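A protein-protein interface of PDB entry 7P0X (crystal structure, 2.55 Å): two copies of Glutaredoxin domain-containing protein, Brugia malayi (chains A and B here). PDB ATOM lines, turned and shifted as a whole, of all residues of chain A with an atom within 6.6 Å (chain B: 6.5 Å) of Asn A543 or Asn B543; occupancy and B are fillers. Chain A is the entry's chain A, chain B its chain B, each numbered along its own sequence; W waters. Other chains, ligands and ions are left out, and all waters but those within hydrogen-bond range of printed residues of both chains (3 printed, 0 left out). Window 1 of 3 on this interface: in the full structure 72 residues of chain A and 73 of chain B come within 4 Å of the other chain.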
ATOM      1  N   LEU A 169      -7.560 -16.951 -37.007  1.00  0.00           N
ATOM      2  CA  LEU A 169      -7.936 -18.280 -36.429  1.00  0.00           C
ATOM      3  C   LEU A 169      -8.674 -19.141 -37.491  1.00  0.00           C
ATOM      4  O   LEU A 169      -8.348 -20.356 -37.651  1.00  0.00           O
ATOM      5  CB  LEU A 169      -8.807 -18.061 -35.187  1.00  0.00           C
ATOM      6  CG  LEU A 169      -8.122 -17.359 -34.027  1.00  0.00           C
ATOM      7  CD1 LEU A 169      -9.124 -17.010 -32.926  1.00  0.00           C
ATOM      8  CD2 LEU A 169      -6.987 -18.200 -33.485  1.00  0.00           C
ATOM      9  N   TYR A 173      -8.359 -22.953 -38.766  1.00  0.00           N
ATOM     10  CA  TYR A 173      -9.529 -23.864 -38.625  1.00  0.00           C
ATOM     11  C   TYR A 173      -9.793 -24.606 -39.940  1.00  0.00           C
ATOM     12  O   TYR A 173     -10.157 -25.833 -39.890  1.00  0.00           O
ATOM     13  CB  TYR A 173     -10.749 -23.119 -38.095  1.00  0.00           C
ATOM     14  CG  TYR A 173     -10.760 -22.907 -36.603  1.00  0.00           C
ATOM     15  CD1 TYR A 173     -10.401 -23.924 -35.735  1.00  0.00           C
ATOM     16  CD2 TYR A 173     -11.214 -21.720 -36.044  1.00  0.00           C
ATOM     17  CE1 TYR A 173     -10.450 -23.758 -34.354  1.00  0.00           C
ATOM     18  CE2 TYR A 173     -11.246 -21.519 -34.668  1.00  0.00           C
ATOM     19  CZ  TYR A 173     -10.875 -22.550 -33.820  1.00  0.00           C
ATOM     20  OH  TYR A 173     -10.924 -22.387 -32.472  1.00  0.00           O
ATOM     21  N   THR A 471      -6.450 -10.450 -21.561  1.00  0.00           N
ATOM     22  CA  THR A 471      -6.073 -11.404 -22.614  1.00  0.00           C
ATOM     23  C   THR A 471      -5.374 -10.589 -23.704  1.00  0.00           C
ATOM     24  O   THR A 471      -5.953  -9.589 -24.160  1.00  0.00           O
ATOM     25  CB  THR A 471      -7.306 -12.188 -23.096  1.00  0.00           C
ATOM     26  OG1 THR A 471      -7.814 -12.949 -22.003  1.00  0.00           O
ATOM     27  CG2 THR A 471      -6.967 -13.086 -24.252  1.00  0.00           C
ATOM     28  N   GLU A 477      -3.562 -17.305 -27.714  1.00  0.00           N
ATOM     29  CA  GLU A 477      -4.046 -16.241 -26.821  1.00  0.00           C
ATOM     30  C   GLU A 477      -3.384 -16.372 -25.435  1.00  0.00           C
ATOM     31  O   GLU A 477      -3.096 -17.483 -24.981  1.00  0.00           O
ATOM     32  CB  GLU A 477      -5.567 -16.271 -26.777  1.00  0.00           C
ATOM     33  CG  GLU A 477      -6.211 -16.140 -28.136  1.00  0.00           C
ATOM     34  CD  GLU A 477      -7.733 -16.091 -28.098  1.00  0.00           C
ATOM     35  OE1 GLU A 477      -8.339 -16.435 -27.026  1.00  0.00           O
ATOM     36  OE2 GLU A 477      -8.330 -15.695 -29.143  1.00  0.00           O
ATOM     37  N   GLU A 508      -9.176 -30.313 -29.180  1.00  0.00           N
ATOM     38  CA  GLU A 508      -9.489 -29.827 -30.551  1.00  0.00           C
ATOM     39  C   GLU A 508      -8.262 -29.935 -31.469  1.00  0.00           C
ATOM     40  O   GLU A 508      -8.456 -29.824 -32.709  1.00  0.00           O
ATOM     41  CB  GLU A 508      -9.918 -28.352 -30.494  1.00  0.00           C
ATOM     42  CG  GLU A 508     -11.281 -28.140 -29.868  1.00  0.00           C
ATOM     43  CD  GLU A 508     -11.329 -28.348 -28.352  1.00  0.00           C
ATOM     44  OE1 GLU A 508     -10.323 -27.979 -27.704  1.00  0.00           O
ATOM     45  OE2 GLU A 508     -12.336 -28.940 -27.843  1.00  0.00           O
ATOM     46  N   THR A 541      -3.263 -20.512 -24.497  1.00  0.00           N
ATOM     47  CA  THR A 541      -4.297 -21.458 -24.973  1.00  0.00           C
ATOM     48  C   THR A 541      -5.215 -20.754 -25.956  1.00  0.00           C
ATOM     49  O   THR A 541      -5.379 -19.539 -25.890  1.00  0.00           O
ATOM     50  CB  THR A 541      -5.172 -21.942 -23.815  1.00  0.00           C
ATOM     51  OG1 THR A 541      -6.154 -22.886 -24.273  1.00  0.00           O
ATOM     52  CG2 THR A 541      -5.894 -20.779 -23.174  1.00  0.00           C
ATOM     53  N   PRO A 542      -5.909 -21.492 -26.837  1.00  0.00           N
ATOM     54  CA  PRO A 542      -7.086 -20.943 -27.495  1.00  0.00           C
ATOM     55  C   PRO A 542      -8.116 -20.555 -26.416  1.00  0.00           C
ATOM     56  O   PRO A 542      -8.151 -21.233 -25.407  1.00  0.00           O
ATOM     57  CB  PRO A 542      -7.641 -22.091 -28.361  1.00  0.00           C
ATOM     58  CG  PRO A 542      -7.014 -23.325 -27.780  1.00  0.00           C
ATOM     59  CD  PRO A 542      -5.674 -22.881 -27.206  1.00  0.00           C
ATOM     60  N   ASN A 543      -8.922 -19.514 -26.693  1.00  0.00           N
ATOM     61  CA  ASN A 543     -10.060 -19.068 -25.845  1.00  0.00           C
ATOM     62  C   ASN A 543      -9.581 -18.609 -24.461  1.00  0.00           C
ATOM     63  O   ASN A 543     -10.377 -18.643 -23.525  1.00  0.00           O
ATOM     64  CB  ASN A 543     -11.093 -20.183 -25.777  1.00  0.00           C
ATOM     65  CG  ASN A 543     -11.493 -20.657 -27.155  1.00  0.00           C
ATOM     66  OD1 ASN A 543     -11.401 -21.843 -27.441  1.00  0.00           O
ATOM     67  ND2 ASN A 543     -11.968 -19.744 -27.986  1.00  0.00           N
ATOM     68  N   ALA A 544      -8.352 -18.107 -24.353  1.00  0.00           N
ATOM     69  CA  ALA A 544      -7.743 -17.615 -23.090  1.00  0.00           C
ATOM     70  C   ALA A 544      -8.678 -16.615 -22.412  1.00  0.00           C
ATOM     71  O   ALA A 544      -8.860 -16.700 -21.168  1.00  0.00           O
ATOM     72  CB  ALA A 544      -6.404 -16.986 -23.364  1.00  0.00           C
ATOM     73  N   GLY A 545      -9.243 -15.709 -23.200  1.00  0.00           N
ATOM     74  CA  GLY A 545     -10.211 -14.729 -22.683  1.00  0.00           C
ATOM     75  C   GLY A 545     -11.379 -15.422 -22.003  1.00  0.00           C
ATOM     76  O   GLY A 545     -11.810 -14.986 -20.885  1.00  0.00           O
ATOM     77  N   GLU A 546     -11.909 -16.459 -22.629  1.00  0.00           N
ATOM     78  CA  GLU A 546     -13.161 -17.060 -22.133  1.00  0.00           C
ATOM     79  C   GLU A 546     -12.826 -17.815 -20.844  1.00  0.00           C
ATOM     80  O   GLU A 546     -13.674 -17.955 -20.004  1.00  0.00           O
ATOM     81  CB  GLU A 546     -13.799 -17.937 -23.214  1.00  0.00           C
ATOM     82  CG  GLU A 546     -14.149 -17.206 -24.493  1.00  0.00           C
ATOM     83  CD  GLU A 546     -15.272 -16.176 -24.418  1.00  0.00           C
ATOM     84  OE1 GLU A 546     -15.906 -16.083 -23.366  1.00  0.00           O
ATOM     85  OE2 GLU A 546     -15.577 -15.504 -25.453  1.00  0.00           O
ATOM     86  N   ILE A 547     -11.616 -18.319 -20.720  1.00  0.00           N
ATOM     87  CA  ILE A 547     -11.193 -19.159 -19.571  1.00  0.00           C
ATOM     88  C   ILE A 547     -10.861 -18.231 -18.409  1.00  0.00           C
ATOM     89  O   ILE A 547     -11.321 -18.525 -17.292  1.00  0.00           O
ATOM     90  CB  ILE A 547     -10.001 -20.042 -19.970  1.00  0.00           C
ATOM     91  CG1 ILE A 547     -10.420 -21.046 -21.041  1.00  0.00           C
ATOM     92  CG2 ILE A 547      -9.370 -20.718 -18.772  1.00  0.00           C
ATOM     93  CD1 ILE A 547      -9.266 -21.580 -21.829  1.00  0.00           C
ATOM     94  N   THR A 548     -10.126 -17.154 -18.687  1.00  0.00           N
ATOM     95  CA  THR A 548      -9.557 -16.259 -17.659  1.00  0.00           C
ATOM     96  C   THR A 548     -10.677 -15.519 -16.901  1.00  0.00           C
ATOM     97  O   THR A 548     -10.517 -15.252 -15.691  1.00  0.00           O
ATOM     98  CB  THR A 548      -8.549 -15.338 -18.346  1.00  0.00           C
ATOM     99  OG1 THR A 548      -7.561 -16.200 -18.921  1.00  0.00           O
ATOM    100  CG2 THR A 548      -7.937 -14.328 -17.404  1.00  0.00           C
ATOM    101  N   LEU B 169     -18.505 -28.351 -35.495  1.00  0.00           N
ATOM    102  CA  LEU B 169     -18.197 -26.897 -35.398  1.00  0.00           C
ATOM    103  C   LEU B 169     -17.320 -26.461 -36.590  1.00  0.00           C
ATOM    104  O   LEU B 169     -17.601 -25.378 -37.218  1.00  0.00           O
ATOM    105  CB  LEU B 169     -17.496 -26.614 -34.066  1.00  0.00           C
ATOM    106  CG  LEU B 169     -18.336 -26.855 -32.814  1.00  0.00           C
ATOM    107  CD1 LEU B 169     -17.504 -26.638 -31.553  1.00  0.00           C
ATOM    108  CD2 LEU B 169     -19.590 -26.007 -32.789  1.00  0.00           C
ATOM    109  N   TYR B 173     -17.441 -23.359 -39.167  1.00  0.00           N
ATOM    110  CA  TYR B 173     -16.265 -22.443 -39.254  1.00  0.00           C
ATOM    111  C   TYR B 173     -15.852 -22.218 -40.715  1.00  0.00           C
ATOM    112  O   TYR B 173     -15.473 -21.056 -41.067  1.00  0.00           O
ATOM    113  CB  TYR B 173     -15.114 -22.906 -38.352  1.00  0.00           C
ATOM    114  CG  TYR B 173     -15.295 -22.541 -36.895  1.00  0.00           C
ATOM    115  CD1 TYR B 173     -15.820 -21.306 -36.530  1.00  0.00           C
ATOM    116  CD2 TYR B 173     -14.954 -23.419 -35.870  1.00  0.00           C
ATOM    117  CE1 TYR B 173     -15.983 -20.956 -35.205  1.00  0.00           C
ATOM    118  CE2 TYR B 173     -15.135 -23.091 -34.533  1.00  0.00           C
ATOM    119  CZ  TYR B 173     -15.631 -21.841 -34.206  1.00  0.00           C
ATOM    120  OH  TYR B 173     -15.843 -21.437 -32.917  1.00  0.00           O
ATOM    121  N   THR B 471     -21.353 -28.852 -18.932  1.00  0.00           N
ATOM    122  CA  THR B 471     -21.621 -28.361 -20.278  1.00  0.00           C
ATOM    123  C   THR B 471     -22.223 -29.521 -21.055  1.00  0.00           C
ATOM    124  O   THR B 471     -21.648 -30.585 -21.013  1.00  0.00           O
ATOM    125  CB  THR B 471     -20.349 -27.754 -20.863  1.00  0.00           C
ATOM    126  OG1 THR B 471     -19.995 -26.612 -20.063  1.00  0.00           O
ATOM    127  CG2 THR B 471     -20.556 -27.343 -22.298  1.00  0.00           C
ATOM    128  N   GLU B 477     -23.463 -24.728 -27.399  1.00  0.00           N
ATOM    129  CA  GLU B 477     -23.113 -25.403 -26.137  1.00  0.00           C
ATOM    130  C   GLU B 477     -23.925 -24.794 -24.967  1.00  0.00           C
ATOM    131  O   GLU B 477     -24.242 -23.601 -24.992  1.00  0.00           O
ATOM    132  CB  GLU B 477     -21.598 -25.353 -25.942  1.00  0.00           C
ATOM    133  CG  GLU B 477     -20.822 -25.938 -27.079  1.00  0.00           C
ATOM    134  CD  GLU B 477     -19.309 -25.894 -26.895  1.00  0.00           C
ATOM    135  OE1 GLU B 477     -18.797 -25.253 -25.894  1.00  0.00           O
ATOM    136  OE2 GLU B 477     -18.636 -26.427 -27.808  1.00  0.00           O
ATOM    137  N   GLU B 508     -17.483 -13.042 -32.897  1.00  0.00           N
ATOM    138  CA  GLU B 508     -17.087 -13.984 -33.992  1.00  0.00           C
ATOM    139  C   GLU B 508     -18.232 -14.196 -34.990  1.00  0.00           C
ATOM    140  O   GLU B 508     -17.940 -14.693 -36.111  1.00  0.00           O
ATOM    141  CB  GLU B 508     -16.713 -15.378 -33.451  1.00  0.00           C
ATOM    142  CG  GLU B 508     -15.433 -15.389 -32.679  1.00  0.00           C
ATOM    143  CD  GLU B 508     -15.536 -14.738 -31.290  1.00  0.00           C
ATOM    144  OE1 GLU B 508     -16.650 -14.837 -30.676  1.00  0.00           O
ATOM    145  OE2 GLU B 508     -14.503 -14.089 -30.852  1.00  0.00           O
ATOM    146  N   THR B 541     -24.043 -20.599 -25.586  1.00  0.00           N
ATOM    147  CA  THR B 541     -22.959 -19.884 -26.285  1.00  0.00           C
ATOM    148  C   THR B 541     -21.963 -20.888 -26.865  1.00  0.00           C
ATOM    149  O   THR B 541     -21.821 -21.989 -26.361  1.00  0.00           O
ATOM    150  CB  THR B 541     -22.196 -18.999 -25.293  1.00  0.00           C
ATOM    151  OG1 THR B 541     -21.154 -18.259 -25.955  1.00  0.00           O
ATOM    152  CG2 THR B 541     -21.579 -19.835 -24.201  1.00  0.00           C
ATOM    153  N   PRO B 542     -21.151 -20.508 -27.856  1.00  0.00           N
ATOM    154  CA  PRO B 542     -19.904 -21.204 -28.120  1.00  0.00           C
ATOM    155  C   PRO B 542     -19.008 -21.142 -26.879  1.00  0.00           C
ATOM    156  O   PRO B 542     -19.087 -20.169 -26.180  1.00  0.00           O
ATOM    157  CB  PRO B 542     -19.248 -20.456 -29.290  1.00  0.00           C
ATOM    158  CG  PRO B 542     -19.931 -19.100 -29.277  1.00  0.00           C
ATOM    159  CD  PRO B 542     -21.323 -19.340 -28.726  1.00  0.00           C
ATOM    160  N   ASN B 543     -18.208 -22.193 -26.667  1.00  0.00           N
ATOM    161  CA  ASN B 543     -17.194 -22.322 -25.601  1.00  0.00           C
ATOM    162  C   ASN B 543     -17.829 -22.236 -24.202  1.00  0.00           C
ATOM    163  O   ASN B 543     -17.130 -21.869 -23.264  1.00  0.00           O
ATOM    164  CB  ASN B 543     -16.114 -21.283 -25.839  1.00  0.00           C
ATOM    165  CG  ASN B 543     -15.568 -21.400 -27.238  1.00  0.00           C
ATOM    166  OD1 ASN B 543     -15.625 -20.449 -28.005  1.00  0.00           O
ATOM    167  ND2 ASN B 543     -15.071 -22.584 -27.581  1.00  0.00           N
ATOM    168  N   ALA B 544     -19.062 -22.693 -24.057  1.00  0.00           N
ATOM    169  CA  ALA B 544     -19.814 -22.702 -22.785  1.00  0.00           C
ATOM    170  C   ALA B 544     -18.982 -23.367 -21.676  1.00  0.00           C
ATOM    171  O   ALA B 544     -18.932 -22.838 -20.545  1.00  0.00           O
ATOM    172  CB  ALA B 544     -21.123 -23.416 -22.991  1.00  0.00           C
ATOM    173  N   GLY B 545     -18.348 -24.488 -21.997  1.00  0.00           N
ATOM    174  CA  GLY B 545     -17.472 -25.192 -21.053  1.00  0.00           C
ATOM    175  C   GLY B 545     -16.364 -24.285 -20.581  1.00  0.00           C
ATOM    176  O   GLY B 545     -16.068 -24.276 -19.390  1.00  0.00           O
ATOM    177  N   GLU B 546     -15.744 -23.532 -21.481  1.00  0.00           N
ATOM    178  CA  GLU B 546     -14.528 -22.771 -21.103  1.00  0.00           C
ATOM    179  C   GLU B 546     -14.988 -21.580 -20.236  1.00  0.00           C
ATOM    180  O   GLU B 546     -14.254 -21.154 -19.390  1.00  0.00           O
ATOM    181  CB  GLU B 546     -13.763 -22.354 -22.355  1.00  0.00           C
ATOM    182  CG  GLU B 546     -13.347 -23.489 -23.278  1.00  0.00           C
ATOM    183  CD  GLU B 546     -12.274 -24.453 -22.781  1.00  0.00           C
ATOM    184  OE1 GLU B 546     -11.707 -24.211 -21.660  1.00  0.00           O
ATOM    185  OE2 GLU B 546     -11.968 -25.451 -23.545  1.00  0.00           O
ATOM    186  N   ILE B 547     -16.198 -21.084 -20.442  1.00  0.00           N
ATOM    187  CA  ILE B 547     -16.747 -19.923 -19.722  1.00  0.00           C
ATOM    188  C   ILE B 547     -17.205 -20.379 -18.342  1.00  0.00           C
ATOM    189  O   ILE B 547     -16.904 -19.676 -17.361  1.00  0.00           O
ATOM    190  CB  ILE B 547     -17.873 -19.278 -20.536  1.00  0.00           C
ATOM    191  CG1 ILE B 547     -17.330 -18.706 -21.839  1.00  0.00           C
ATOM    192  CG2 ILE B 547     -18.591 -18.215 -19.730  1.00  0.00           C
ATOM    193  CD1 ILE B 547     -18.380 -18.507 -22.871  1.00  0.00           C
ATOM    194  N   THR B 548     -17.912 -21.505 -18.284  1.00  0.00           N
ATOM    195  CA  THR B 548     -18.630 -21.962 -17.069  1.00  0.00           C
ATOM    196  C   THR B 548     -17.621 -22.375 -15.987  1.00  0.00           C
ATOM    197  O   THR B 548     -17.909 -22.183 -14.790  1.00  0.00           O
ATOM    198  CB  THR B 548     -19.585 -23.069 -17.487  1.00  0.00           C
ATOM    199  OG1 THR B 548     -20.507 -22.468 -18.397  1.00  0.00           O
ATOM    200  CG2 THR B 548     -20.326 -23.693 -16.332  1.00  0.00           C
HETATM  201  O   HOH W   1     -10.530 -24.029 -25.639  1.00  0.00           O
HETATM  202  O   HOH W   2     -13.210 -20.621 -17.005  1.00  0.00           O
HETATM  203  O   HOH W   3     -11.135 -28.330 -25.036  1.00  0.00           O
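Water W2 bridges O of Glu B546 and O of Ile A547.
Water W3 lies within hydrogen-bond range of OE1 of Glu A508 (2.8 Å) and OE2 of Glu B546 (3.3 Å).
Water W1 bridges the side-chain carboxylate (OE2) of Glu B546 (2.9 Å) and the side-chain amide oxygen (OD1) of Asn A543 (3.0 Å).
Asn B543 touches its own counterpart, Asn A543.
Glu B546 touches its own counterpart, Glu A546.
Glu A546 touches Ile B547, and with the chains exchanged Ile A547 touches Glu B546.
Thr A471 touches none of the printed residues of chain B.
Asn A543 touches just one residue of chain B: Asn B543 (3.7 Å).
Gly A545 touches none of the printed residues of chain B.
Of the printed residues of chain B, Glu A546 touches Glu B546 (3.3 Å) and Ile B547 (3.4 Å).
Of the printed residues of chain B, Ile A547 touches Glu B546.
Of the printed residues of chain A, Glu B546 touches Glu A546 and Ile A547.
Printed residues of chain A within 4 Å of Ile B547: Glu A546.
The nearest residue of chain B that does not touch Asn A543 is Glu B546 (4.7 Å).
The nearest residue of chain A that does not touch Asn B543 is Glu A546 (4.7 Å).
The backbone carbonyl oxygen of Glu B546 sits close to the backbone carbonyl oxygen of Glu A546 (3.3 Å).
Among the printed residues, merely in contact across the chains: Glu A546 with Ile B547 (3.4 Å), Ile A547 with Glu B546 (3.5 Å) and Asn A543 with Asn B543 (3.7 Å).
Hydrophobic or aromatic side chains of chain A within 4 Å of the printed part of chain B: Ile A547.
Along chain A the printed residues that touch a printed residue of chain B span positions 543 to 547.
Along chain B the printed residues that touch a printed residue of chain A span positions 543 to 547.
N of Asn A543 sits at hydrogen-bond distance from OE1 of Glu A477, at 3.2 Å.
The side-chain carboxylate (OE1) of Glu B477 is in hydrogen-bond range of the backbone NH (N) of Asn B543, at 3.2 Å.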
